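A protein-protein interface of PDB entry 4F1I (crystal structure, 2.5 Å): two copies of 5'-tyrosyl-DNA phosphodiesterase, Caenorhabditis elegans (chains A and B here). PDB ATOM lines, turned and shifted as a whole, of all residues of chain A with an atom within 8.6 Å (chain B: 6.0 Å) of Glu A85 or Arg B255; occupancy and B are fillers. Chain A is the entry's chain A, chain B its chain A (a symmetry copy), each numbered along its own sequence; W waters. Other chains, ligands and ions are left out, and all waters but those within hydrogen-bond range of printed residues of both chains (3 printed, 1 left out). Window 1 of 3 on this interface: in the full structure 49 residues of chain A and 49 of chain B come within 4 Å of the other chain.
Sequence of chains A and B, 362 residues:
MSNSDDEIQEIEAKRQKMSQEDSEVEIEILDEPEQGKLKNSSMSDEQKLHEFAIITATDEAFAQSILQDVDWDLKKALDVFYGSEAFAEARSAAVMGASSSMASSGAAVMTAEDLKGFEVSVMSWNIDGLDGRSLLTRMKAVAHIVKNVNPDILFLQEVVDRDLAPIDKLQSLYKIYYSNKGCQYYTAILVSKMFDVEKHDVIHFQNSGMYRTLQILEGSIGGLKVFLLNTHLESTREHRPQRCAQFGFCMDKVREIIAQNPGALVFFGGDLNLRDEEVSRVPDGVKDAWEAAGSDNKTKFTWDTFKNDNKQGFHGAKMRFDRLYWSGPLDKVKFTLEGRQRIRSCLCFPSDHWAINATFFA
Water W3 lies within hydrogen-bond range of OD2 of Asp B252 and O of Ala A88.
Water W1 lies within hydrogen-bond range of the backbone carbonyl oxygen (O) of Asp A79 (2.7 Å), the backbone NH (N) of Arg B281 (3.2 Å) and the backbone NH (N) of Gly A83 (3.4 Å).
Water W2 lies within hydrogen-bond range of O of Tyr A82 (2.7 Å) and OD1 of Asp B252 (3.5 Å).
The backbone carbonyl oxygen (O) of Ala A259 sits close to the backbone carbonyl oxygen (O) of Ala B259 (3.2 Å).
The guanidinium group (NH1) of Arg B255 lies within salt-bridge range of the side-chain carboxylate (OE2) of Glu A85, at 3.4 Å.
The side-chain carboxylate (OD2) of Asp B252 lies within salt-bridge range of the guanidinium group (NE) of Arg A91 (2.7 Å).
Hydrophobic or aromatic side chains of chain A within 4 Å of the printed part of chain B: Ala A88.
Among the printed residues, 6 pairs touch across the chains.
Among the printed residues, Asp or Glu carboxylates within 4 Å of a Lys or Arg side-chain nitrogen of the other chain: Glu A85 with Arg B255 (3.4 Å) and Arg A91 with Asp B252 (2.7 Å).
The backbone carbonyl oxygen (O) of Tyr A82 lies within hydrogen-bond range of the guanidinium group (NH1) of Arg A91 (3.2 Å).
O of Phe A81 is in hydrogen-bond range of NH1 of Arg A91, at 2.7 Å.
The guanidinium group (NH2) of Arg A91 is in hydrogen-bond range of the backbone carbonyl oxygen (O) of Ser A84, 2.7 Å away.
The side-chain carboxylate (OD1) of Asp B252 lies within salt-bridge range of the guanidinium group (NH2) of Arg B255.
NE2 of Gln B260 sits close to O of Glu B256 (3.4 Å).
Arg B281 touches Gly A83 (NE to O, 3.99 Å).
OD2 of Asp B252 touches CA of Ala A88 (3.5 Å).
Gln B260 touches Ala A259.
Ala B259 touches its own counterpart, Ala A259.
1 position is printed for both chains.
Of the 6 pairs that touch across the chains among the printed residues, 1 has its exchanged pair printed and touching as well.
Of the printed residues of chain B, Gly A83 touches Arg B281 (3.99 Å).
Of chain B, only Arg B255 (3.4 Å) comes within 4 Å of Glu A85.
Printed residues of chain B within 4 Å of Ala A88: Asp B252 (3.5 Å).
Of the printed residues of chain A, Asp B252 touches Ala A88 and Arg A91.
Lys B253 touches none of the printed residues of chain A.
Arg B255 touches one residue of chain A.
Of the printed residues of chain A, Gln B260 touches Ala A259.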
ATOM      1  N   ASP A  79     -15.020   6.086  -1.557  1.00  0.00           N
ATOM      2  CA  ASP A  79     -13.736   6.641  -1.142  1.00  0.00           C
ATOM      3  C   ASP A  79     -12.954   5.645  -0.301  1.00  0.00           C
ATOM      4  O   ASP A  79     -11.726   5.610  -0.347  1.00  0.00           O
ATOM      5  CB  ASP A  79     -13.949   7.929  -0.344  1.00  0.00           C
ATOM      6  CG  ASP A  79     -14.594   9.027  -1.168  1.00  0.00           C
ATOM      7  OD1 ASP A  79     -14.676  10.171  -0.672  1.00  0.00           O
ATOM      8  OD2 ASP A  79     -15.010   8.748  -2.314  1.00  0.00           O
ATOM      9  N   VAL A  80     -13.672   4.837   0.471  1.00  0.00           N
ATOM     10  CA  VAL A  80     -13.045   3.818   1.293  1.00  0.00           C
ATOM     11  C   VAL A  80     -12.528   2.688   0.413  1.00  0.00           C
ATOM     12  O   VAL A  80     -11.402   2.229   0.575  1.00  0.00           O
ATOM     13  CB  VAL A  80     -14.031   3.245   2.329  1.00  0.00           C
ATOM     14  CG1 VAL A  80     -13.289   2.403   3.344  1.00  0.00           C
ATOM     15  CG2 VAL A  80     -14.774   4.365   3.029  1.00  0.00           C
ATOM     16  N   PHE A  81     -13.352   2.243  -0.529  1.00  0.00           N
ATOM     17  CA  PHE A  81     -12.957   1.149  -1.407  1.00  0.00           C
ATOM     18  C   PHE A  81     -11.733   1.496  -2.249  1.00  0.00           C
ATOM     19  O   PHE A  81     -10.843   0.665  -2.427  1.00  0.00           O
ATOM     20  CB  PHE A  81     -14.110   0.731  -2.316  1.00  0.00           C
ATOM     21  CG  PHE A  81     -13.717  -0.271  -3.359  1.00  0.00           C
ATOM     22  CD1 PHE A  81     -13.271  -1.529  -2.994  1.00  0.00           C
ATOM     23  CD2 PHE A  81     -13.794   0.042  -4.706  1.00  0.00           C
ATOM     24  CE1 PHE A  81     -12.905  -2.455  -3.949  1.00  0.00           C
ATOM     25  CE2 PHE A  81     -13.434  -0.882  -5.667  1.00  0.00           C
ATOM     26  CZ  PHE A  81     -12.988  -2.132  -5.287  1.00  0.00           C
ATOM     27  N   TYR A  82     -11.686   2.723  -2.755  1.00  0.00           N
ATOM     28  CA  TYR A  82     -10.590   3.125  -3.634  1.00  0.00           C
ATOM     29  C   TYR A  82      -9.357   3.639  -2.891  1.00  0.00           C
ATOM     30  O   TYR A  82      -8.230   3.360  -3.294  1.00  0.00           O
ATOM     31  CB  TYR A  82     -11.060   4.157  -4.671  1.00  0.00           C
ATOM     32  CG  TYR A  82     -12.025   3.592  -5.687  1.00  0.00           C
ATOM     33  CD1 TYR A  82     -11.624   2.597  -6.570  1.00  0.00           C
ATOM     34  CD2 TYR A  82     -13.333   4.046  -5.762  1.00  0.00           C
ATOM     35  CE1 TYR A  82     -12.498   2.069  -7.498  1.00  0.00           C
ATOM     36  CE2 TYR A  82     -14.219   3.521  -6.688  1.00  0.00           C
ATOM     37  CZ  TYR A  82     -13.795   2.532  -7.555  1.00  0.00           C
ATOM     38  OH  TYR A  82     -14.661   1.996  -8.483  1.00  0.00           O
ATOM     39  N   GLY A  83      -9.572   4.374  -1.804  1.00  0.00           N
ATOM     40  CA  GLY A  83      -8.491   5.087  -1.146  1.00  0.00           C
ATOM     41  C   GLY A  83      -8.024   4.559   0.200  1.00  0.00           C
ATOM     42  O   GLY A  83      -6.893   4.825   0.605  1.00  0.00           O
ATOM     43  N   SER A  84      -8.880   3.827   0.906  1.00  0.00           N
ATOM     44  CA  SER A  84      -8.507   3.316   2.223  1.00  0.00           C
ATOM     45  C   SER A  84      -7.456   2.209   2.145  1.00  0.00           C
ATOM     46  O   SER A  84      -7.473   1.381   1.235  1.00  0.00           O
ATOM     47  CB  SER A  84      -9.734   2.837   2.999  1.00  0.00           C
ATOM     48  OG  SER A  84      -9.356   2.053   4.116  1.00  0.00           O
ATOM     49  N   GLU A  85      -6.550   2.203   3.115  1.00  0.00           N
ATOM     50  CA  GLU A  85      -5.430   1.270   3.127  1.00  0.00           C
ATOM     51  C   GLU A  85      -5.873  -0.150   3.474  1.00  0.00           C
ATOM     52  O   GLU A  85      -5.192  -1.123   3.151  1.00  0.00           O
ATOM     53  CB  GLU A  85      -4.366   1.751   4.114  1.00  0.00           C
ATOM     54  CG  GLU A  85      -3.074   0.963   4.080  1.00  0.00           C
ATOM     55  CD  GLU A  85      -2.034   1.505   5.043  1.00  0.00           C
ATOM     56  OE1 GLU A  85      -2.267   2.585   5.629  1.00  0.00           O
ATOM     57  OE2 GLU A  85      -0.986   0.846   5.213  1.00  0.00           O
ATOM     58  N   ALA A  86      -7.024  -0.262   4.125  1.00  0.00           N
ATOM     59  CA  ALA A  86      -7.543  -1.558   4.537  1.00  0.00           C
ATOM     60  C   ALA A  86      -7.932  -2.428   3.345  1.00  0.00           C
ATOM     61  O   ALA A  86      -7.844  -3.655   3.408  1.00  0.00           O
ATOM     62  CB  ALA A  86      -8.732  -1.374   5.464  1.00  0.00           C
ATOM     63  N   PHE A  87      -8.349  -1.791   2.256  1.00  0.00           N
ATOM     64  CA  PHE A  87      -8.930  -2.521   1.131  1.00  0.00           C
ATOM     65  C   PHE A  87      -7.977  -2.790  -0.029  1.00  0.00           C
ATOM     66  O   PHE A  87      -8.417  -3.181  -1.117  1.00  0.00           O
ATOM     67  CB  PHE A  87     -10.185  -1.812   0.630  1.00  0.00           C
ATOM     68  CG  PHE A  87     -11.346  -1.929   1.567  1.00  0.00           C
ATOM     69  CD1 PHE A  87     -12.070  -3.105   1.639  1.00  0.00           C
ATOM     70  CD2 PHE A  87     -11.706  -0.874   2.385  1.00  0.00           C
ATOM     71  CE1 PHE A  87     -13.137  -3.225   2.503  1.00  0.00           C
ATOM     72  CE2 PHE A  87     -12.774  -0.989   3.252  1.00  0.00           C
ATOM     73  CZ  PHE A  87     -13.490  -2.166   3.309  1.00  0.00           C
ATOM     74  N   ALA A  88      -6.682  -2.595   0.213  1.00  0.00           N
ATOM     75  CA  ALA A  88      -5.654  -2.881  -0.782  1.00  0.00           C
ATOM     76  C   ALA A  88      -5.867  -4.261  -1.394  1.00  0.00           C
ATOM     77  O   ALA A  88      -5.933  -4.407  -2.619  1.00  0.00           O
ATOM     78  CB  ALA A  88      -4.275  -2.783  -0.163  1.00  0.00           C
ATOM     79  N   GLU A  89      -6.012  -5.254  -0.520  1.00  0.00           N
ATOM     80  CA  GLU A  89      -6.300  -6.626  -0.916  1.00  0.00           C
ATOM     81  C   GLU A  89      -7.429  -6.663  -1.940  1.00  0.00           C
ATOM     82  O   GLU A  89      -7.255  -7.166  -3.056  1.00  0.00           O
ATOM     83  CB  GLU A  89      -6.685  -7.452   0.313  1.00  0.00           C
ATOM     84  CG  GLU A  89      -6.755  -8.951   0.076  1.00  0.00           C
ATOM     85  CD  GLU A  89      -5.409  -9.636   0.247  1.00  0.00           C
ATOM     86  OE1 GLU A  89      -4.368  -8.950   0.145  1.00  0.00           O
ATOM     87  OE2 GLU A  89      -5.397 -10.863   0.494  1.00  0.00           O
ATOM     88  N   ALA A  90      -8.571  -6.091  -1.563  1.00  0.00           N
ATOM     89  CA  ALA A  90      -9.729  -6.047  -2.443  1.00  0.00           C
ATOM     90  C   ALA A  90      -9.339  -5.444  -3.784  1.00  0.00           C
ATOM     91  O   ALA A  90      -9.606  -6.029  -4.840  1.00  0.00           O
ATOM     92  CB  ALA A  90     -10.852  -5.247  -1.806  1.00  0.00           C
ATOM     93  N   ARG A  91      -8.664  -4.298  -3.733  1.00  0.00           N
ATOM     94  CA  ARG A  91      -8.260  -3.616  -4.954  1.00  0.00           C
ATOM     95  C   ARG A  91      -7.378  -4.522  -5.797  1.00  0.00           C
ATOM     96  O   ARG A  91      -7.550  -4.600  -7.016  1.00  0.00           O
ATOM     97  CB  ARG A  91      -7.559  -2.292  -4.646  1.00  0.00           C
ATOM     98  CG  ARG A  91      -8.514  -1.184  -4.239  1.00  0.00           C
ATOM     99  CD  ARG A  91      -7.814   0.158  -4.154  1.00  0.00           C
ATOM    100  NE  ARG A  91      -6.805   0.178  -3.100  1.00  0.00           N
ATOM    101  CZ  ARG A  91      -7.063   0.449  -1.824  1.00  0.00           C
ATOM    102  NH1 ARG A  91      -8.301   0.727  -1.439  1.00  0.00           N
ATOM    103  NH2 ARG A  91      -6.081   0.444  -0.935  1.00  0.00           N
ATOM    104  N   ALA A 259       8.464  -2.222   8.733  1.00  0.00           N
ATOM    105  CA  ALA A 259       7.937  -1.447   7.617  1.00  0.00           C
ATOM    106  C   ALA A 259       8.838  -1.548   6.394  1.00  0.00           C
ATOM    107  O   ALA A 259       8.364  -1.505   5.255  1.00  0.00           O
ATOM    108  CB  ALA A 259       7.758   0.005   8.019  1.00  0.00           C
ATOM    109  N   CYS B 250      -2.429   1.324  -8.111  1.00  0.00           N
ATOM    110  CA  CYS B 250      -1.136   1.940  -8.368  1.00  0.00           C
ATOM    111  C   CYS B 250      -0.658   2.716  -7.149  1.00  0.00           C
ATOM    112  O   CYS B 250       0.531   2.721  -6.835  1.00  0.00           O
ATOM    113  CB  CYS B 250      -1.219   2.875  -9.572  1.00  0.00           C
ATOM    114  SG  CYS B 250      -1.342   2.038 -11.168  1.00  0.00           S
ATOM    115  N   MET B 251      -1.594   3.372  -6.469  1.00  0.00           N
ATOM    116  CA  MET B 251      -1.275   4.140  -5.270  1.00  0.00           C
ATOM    117  C   MET B 251      -0.903   3.225  -4.108  1.00  0.00           C
ATOM    118  O   MET B 251      -0.176   3.624  -3.200  1.00  0.00           O
ATOM    119  CB  MET B 251      -2.435   5.064  -4.887  1.00  0.00           C
ATOM    120  CG  MET B 251      -2.500   6.350  -5.706  1.00  0.00           C
ATOM    121  SD  MET B 251      -0.814   7.365  -5.681  1.00  0.00           S
ATOM    122  CE  MET B 251      -1.389   8.945  -6.660  1.00  0.00           C
ATOM    123  N   ASP B 252      -1.404   1.994  -4.141  1.00  0.00           N
ATOM    124  CA  ASP B 252      -1.025   0.997  -3.148  1.00  0.00           C
ATOM    125  C   ASP B 252       0.431   0.598  -3.342  1.00  0.00           C
ATOM    126  O   ASP B 252       1.186   0.479  -2.376  1.00  0.00           O
ATOM    127  CB  ASP B 252      -1.915  -0.239  -3.251  1.00  0.00           C
ATOM    128  CG  ASP B 252      -3.325   0.014  -2.754  1.00  0.00           C
ATOM    129  OD1 ASP B 252      -3.513   0.929  -1.920  1.00  0.00           O
ATOM    130  OD2 ASP B 252      -4.244  -0.711  -3.190  1.00  0.00           O
ATOM    131  N   LYS B 253       0.813   0.392  -4.599  1.00  0.00           N
ATOM    132  CA  LYS B 253       2.186   0.044  -4.948  1.00  0.00           C
ATOM    133  C   LYS B 253       3.143   1.161  -4.558  1.00  0.00           C
ATOM    134  O   LYS B 253       4.251   0.904  -4.087  1.00  0.00           O
ATOM    135  CB  LYS B 253       2.299  -0.239  -6.445  1.00  0.00           C
ATOM    136  CG  LYS B 253       1.496  -1.443  -6.890  1.00  0.00           C
ATOM    137  CD  LYS B 253       2.001  -2.706  -6.224  1.00  0.00           C
ATOM    138  CE  LYS B 253       0.913  -3.762  -6.146  1.00  0.00           C
ATOM    139  NZ  LYS B 253       1.442  -5.070  -5.657  1.00  0.00           N
ATOM    140  N   VAL B 254       2.704   2.399  -4.765  1.00  0.00           N
ATOM    141  CA  VAL B 254       3.476   3.572  -4.381  1.00  0.00           C
ATOM    142  C   VAL B 254       3.696   3.597  -2.870  1.00  0.00           C
ATOM    143  O   VAL B 254       4.807   3.848  -2.400  1.00  0.00           O
ATOM    144  CB  VAL B 254       2.779   4.867  -4.842  1.00  0.00           C
ATOM    145  CG1 VAL B 254       3.294   6.076  -4.068  1.00  0.00           C
ATOM    146  CG2 VAL B 254       2.973   5.058  -6.330  1.00  0.00           C
ATOM    147  N   ARG B 255       2.637   3.314  -2.118  1.00  0.00           N
ATOM    148  CA  ARG B 255       2.708   3.270  -0.661  1.00  0.00           C
ATOM    149  C   ARG B 255       3.733   2.258  -0.169  1.00  0.00           C
ATOM    150  O   ARG B 255       4.476   2.524   0.775  1.00  0.00           O
ATOM    151  CB  ARG B 255       1.347   2.925  -0.062  1.00  0.00           C
ATOM    152  CG  ARG B 255       0.539   4.120   0.391  1.00  0.00           C
ATOM    153  CD  ARG B 255      -0.495   3.732   1.445  1.00  0.00           C
ATOM    154  NE  ARG B 255      -1.481   2.783   0.932  1.00  0.00           N
ATOM    155  CZ  ARG B 255      -1.430   1.468   1.128  1.00  0.00           C
ATOM    156  NH1 ARG B 255      -0.441   0.935   1.834  1.00  0.00           N
ATOM    157  NH2 ARG B 255      -2.372   0.688   0.618  1.00  0.00           N
ATOM    158  N   GLU B 256       3.757   1.093  -0.809  1.00  0.00           N
ATOM    159  CA  GLU B 256       4.689   0.037  -0.441  1.00  0.00           C
ATOM    160  C   GLU B 256       6.125   0.489  -0.652  1.00  0.00           C
ATOM    161  O   GLU B 256       6.975   0.327   0.224  1.00  0.00           O
ATOM    162  CB  GLU B 256       4.429  -1.221  -1.265  1.00  0.00           C
ATOM    163  CG  GLU B 256       3.088  -1.874  -1.007  1.00  0.00           C
ATOM    164  CD  GLU B 256       2.908  -3.146  -1.814  1.00  0.00           C
ATOM    165  OE1 GLU B 256       3.804  -3.465  -2.626  1.00  0.00           O
ATOM    166  OE2 GLU B 256       1.875  -3.826  -1.633  1.00  0.00           O
ATOM    167  N   ILE B 257       6.381   1.057  -1.824  1.00  0.00           N
ATOM    168  CA  ILE B 257       7.710   1.528  -2.187  1.00  0.00           C
ATOM    169  C   ILE B 257       8.213   2.592  -1.213  1.00  0.00           C
ATOM    170  O   ILE B 257       9.384   2.595  -0.825  1.00  0.00           O
ATOM    171  CB  ILE B 257       7.714   2.083  -3.626  1.00  0.00           C
ATOM    172  CG1 ILE B 257       7.447   0.947  -4.621  1.00  0.00           C
ATOM    173  CG2 ILE B 257       9.031   2.779  -3.933  1.00  0.00           C
ATOM    174  CD1 ILE B 257       7.292   1.405  -6.059  1.00  0.00           C
ATOM    175  N   ILE B 258       7.315   3.482  -0.806  1.00  0.00           N
ATOM    176  CA  ILE B 258       7.657   4.548   0.125  1.00  0.00           C
ATOM    177  C   ILE B 258       7.940   3.976   1.509  1.00  0.00           C
ATOM    178  O   ILE B 258       8.878   4.396   2.190  1.00  0.00           O
ATOM    179  CB  ILE B 258       6.524   5.594   0.211  1.00  0.00           C
ATOM    180  CG1 ILE B 258       6.375   6.326  -1.126  1.00  0.00           C
ATOM    181  CG2 ILE B 258       6.783   6.599   1.325  1.00  0.00           C
ATOM    182  CD1 ILE B 258       5.164   7.222  -1.176  1.00  0.00           C
ATOM    183  N   ALA B 259       7.134   3.000   1.912  1.00  0.00           N
ATOM    184  CA  ALA B 259       7.273   2.385   3.226  1.00  0.00           C
ATOM    185  C   ALA B 259       8.567   1.590   3.335  1.00  0.00           C
ATOM    186  O   ALA B 259       9.162   1.497   4.412  1.00  0.00           O
ATOM    187  CB  ALA B 259       6.081   1.491   3.519  1.00  0.00           C
ATOM    188  N   GLN B 260       9.006   1.028   2.216  1.00  0.00           N
ATOM    189  CA  GLN B 260      10.167   0.146   2.216  1.00  0.00           C
ATOM    190  C   GLN B 260      11.455   0.857   1.819  1.00  0.00           C
ATOM    191  O   GLN B 260      12.549   0.324   2.002  1.00  0.00           O
ATOM    192  CB  GLN B 260       9.919  -1.053   1.302  1.00  0.00           C
ATOM    193  CG  GLN B 260       8.758  -1.913   1.753  1.00  0.00           C
ATOM    194  CD  GLN B 260       8.287  -2.871   0.679  1.00  0.00           C
ATOM    195  OE1 GLN B 260       9.090  -3.418  -0.077  1.00  0.00           O
ATOM    196  NE2 GLN B 260       6.976  -3.075   0.604  1.00  0.00           N
ATOM    197  N   ARG B 281      -8.109   9.223  -2.580  1.00  0.00           N
ATOM    198  CA  ARG B 281      -7.135   9.702  -1.610  1.00  0.00           C
ATOM    199  C   ARG B 281      -5.725   9.245  -1.965  1.00  0.00           C
ATOM    200  O   ARG B 281      -5.475   8.051  -2.128  1.00  0.00           O
ATOM    201  CB  ARG B 281      -7.493   9.205  -0.207  1.00  0.00           C
ATOM    202  CG  ARG B 281      -6.837   9.987   0.917  1.00  0.00           C
ATOM    203  CD  ARG B 281      -6.844   9.204   2.219  1.00  0.00           C
ATOM    204  NE  ARG B 281      -5.739   8.250   2.287  1.00  0.00           N
ATOM    205  CZ  ARG B 281      -4.561   8.508   2.848  1.00  0.00           C
ATOM    206  NH1 ARG B 281      -4.329   9.694   3.395  1.00  0.00           N
ATOM    207  NH2 ARG B 281      -3.613   7.579   2.863  1.00  0.00           N
ATOM    208  N   PRO B 283      -1.745   8.828  -0.808  1.00  0.00           N
ATOM    209  CA  PRO B 283      -0.989   8.622   0.437  1.00  0.00           C
ATOM    210  C   PRO B 283      -0.230   9.864   0.899  1.00  0.00           C
ATOM    211  O   PRO B 283       0.166  10.681   0.070  1.00  0.00           O
ATOM    212  CB  PRO B 283      -0.002   7.508   0.071  1.00  0.00           C
ATOM    213  CG  PRO B 283      -0.031   7.406  -1.421  1.00  0.00           C
ATOM    214  CD  PRO B 283      -1.395   7.837  -1.836  1.00  0.00           C
HETATM  215  O   HOH W   1     -10.686   7.547  -1.834  1.00  0.00           O
HETATM  216  O   HOH W   2      -5.527   3.515  -3.097  1.00  0.00           O
HETATM  217  O   HOH W   3      -4.039  -3.166  -3.863  1.00  0.00           O
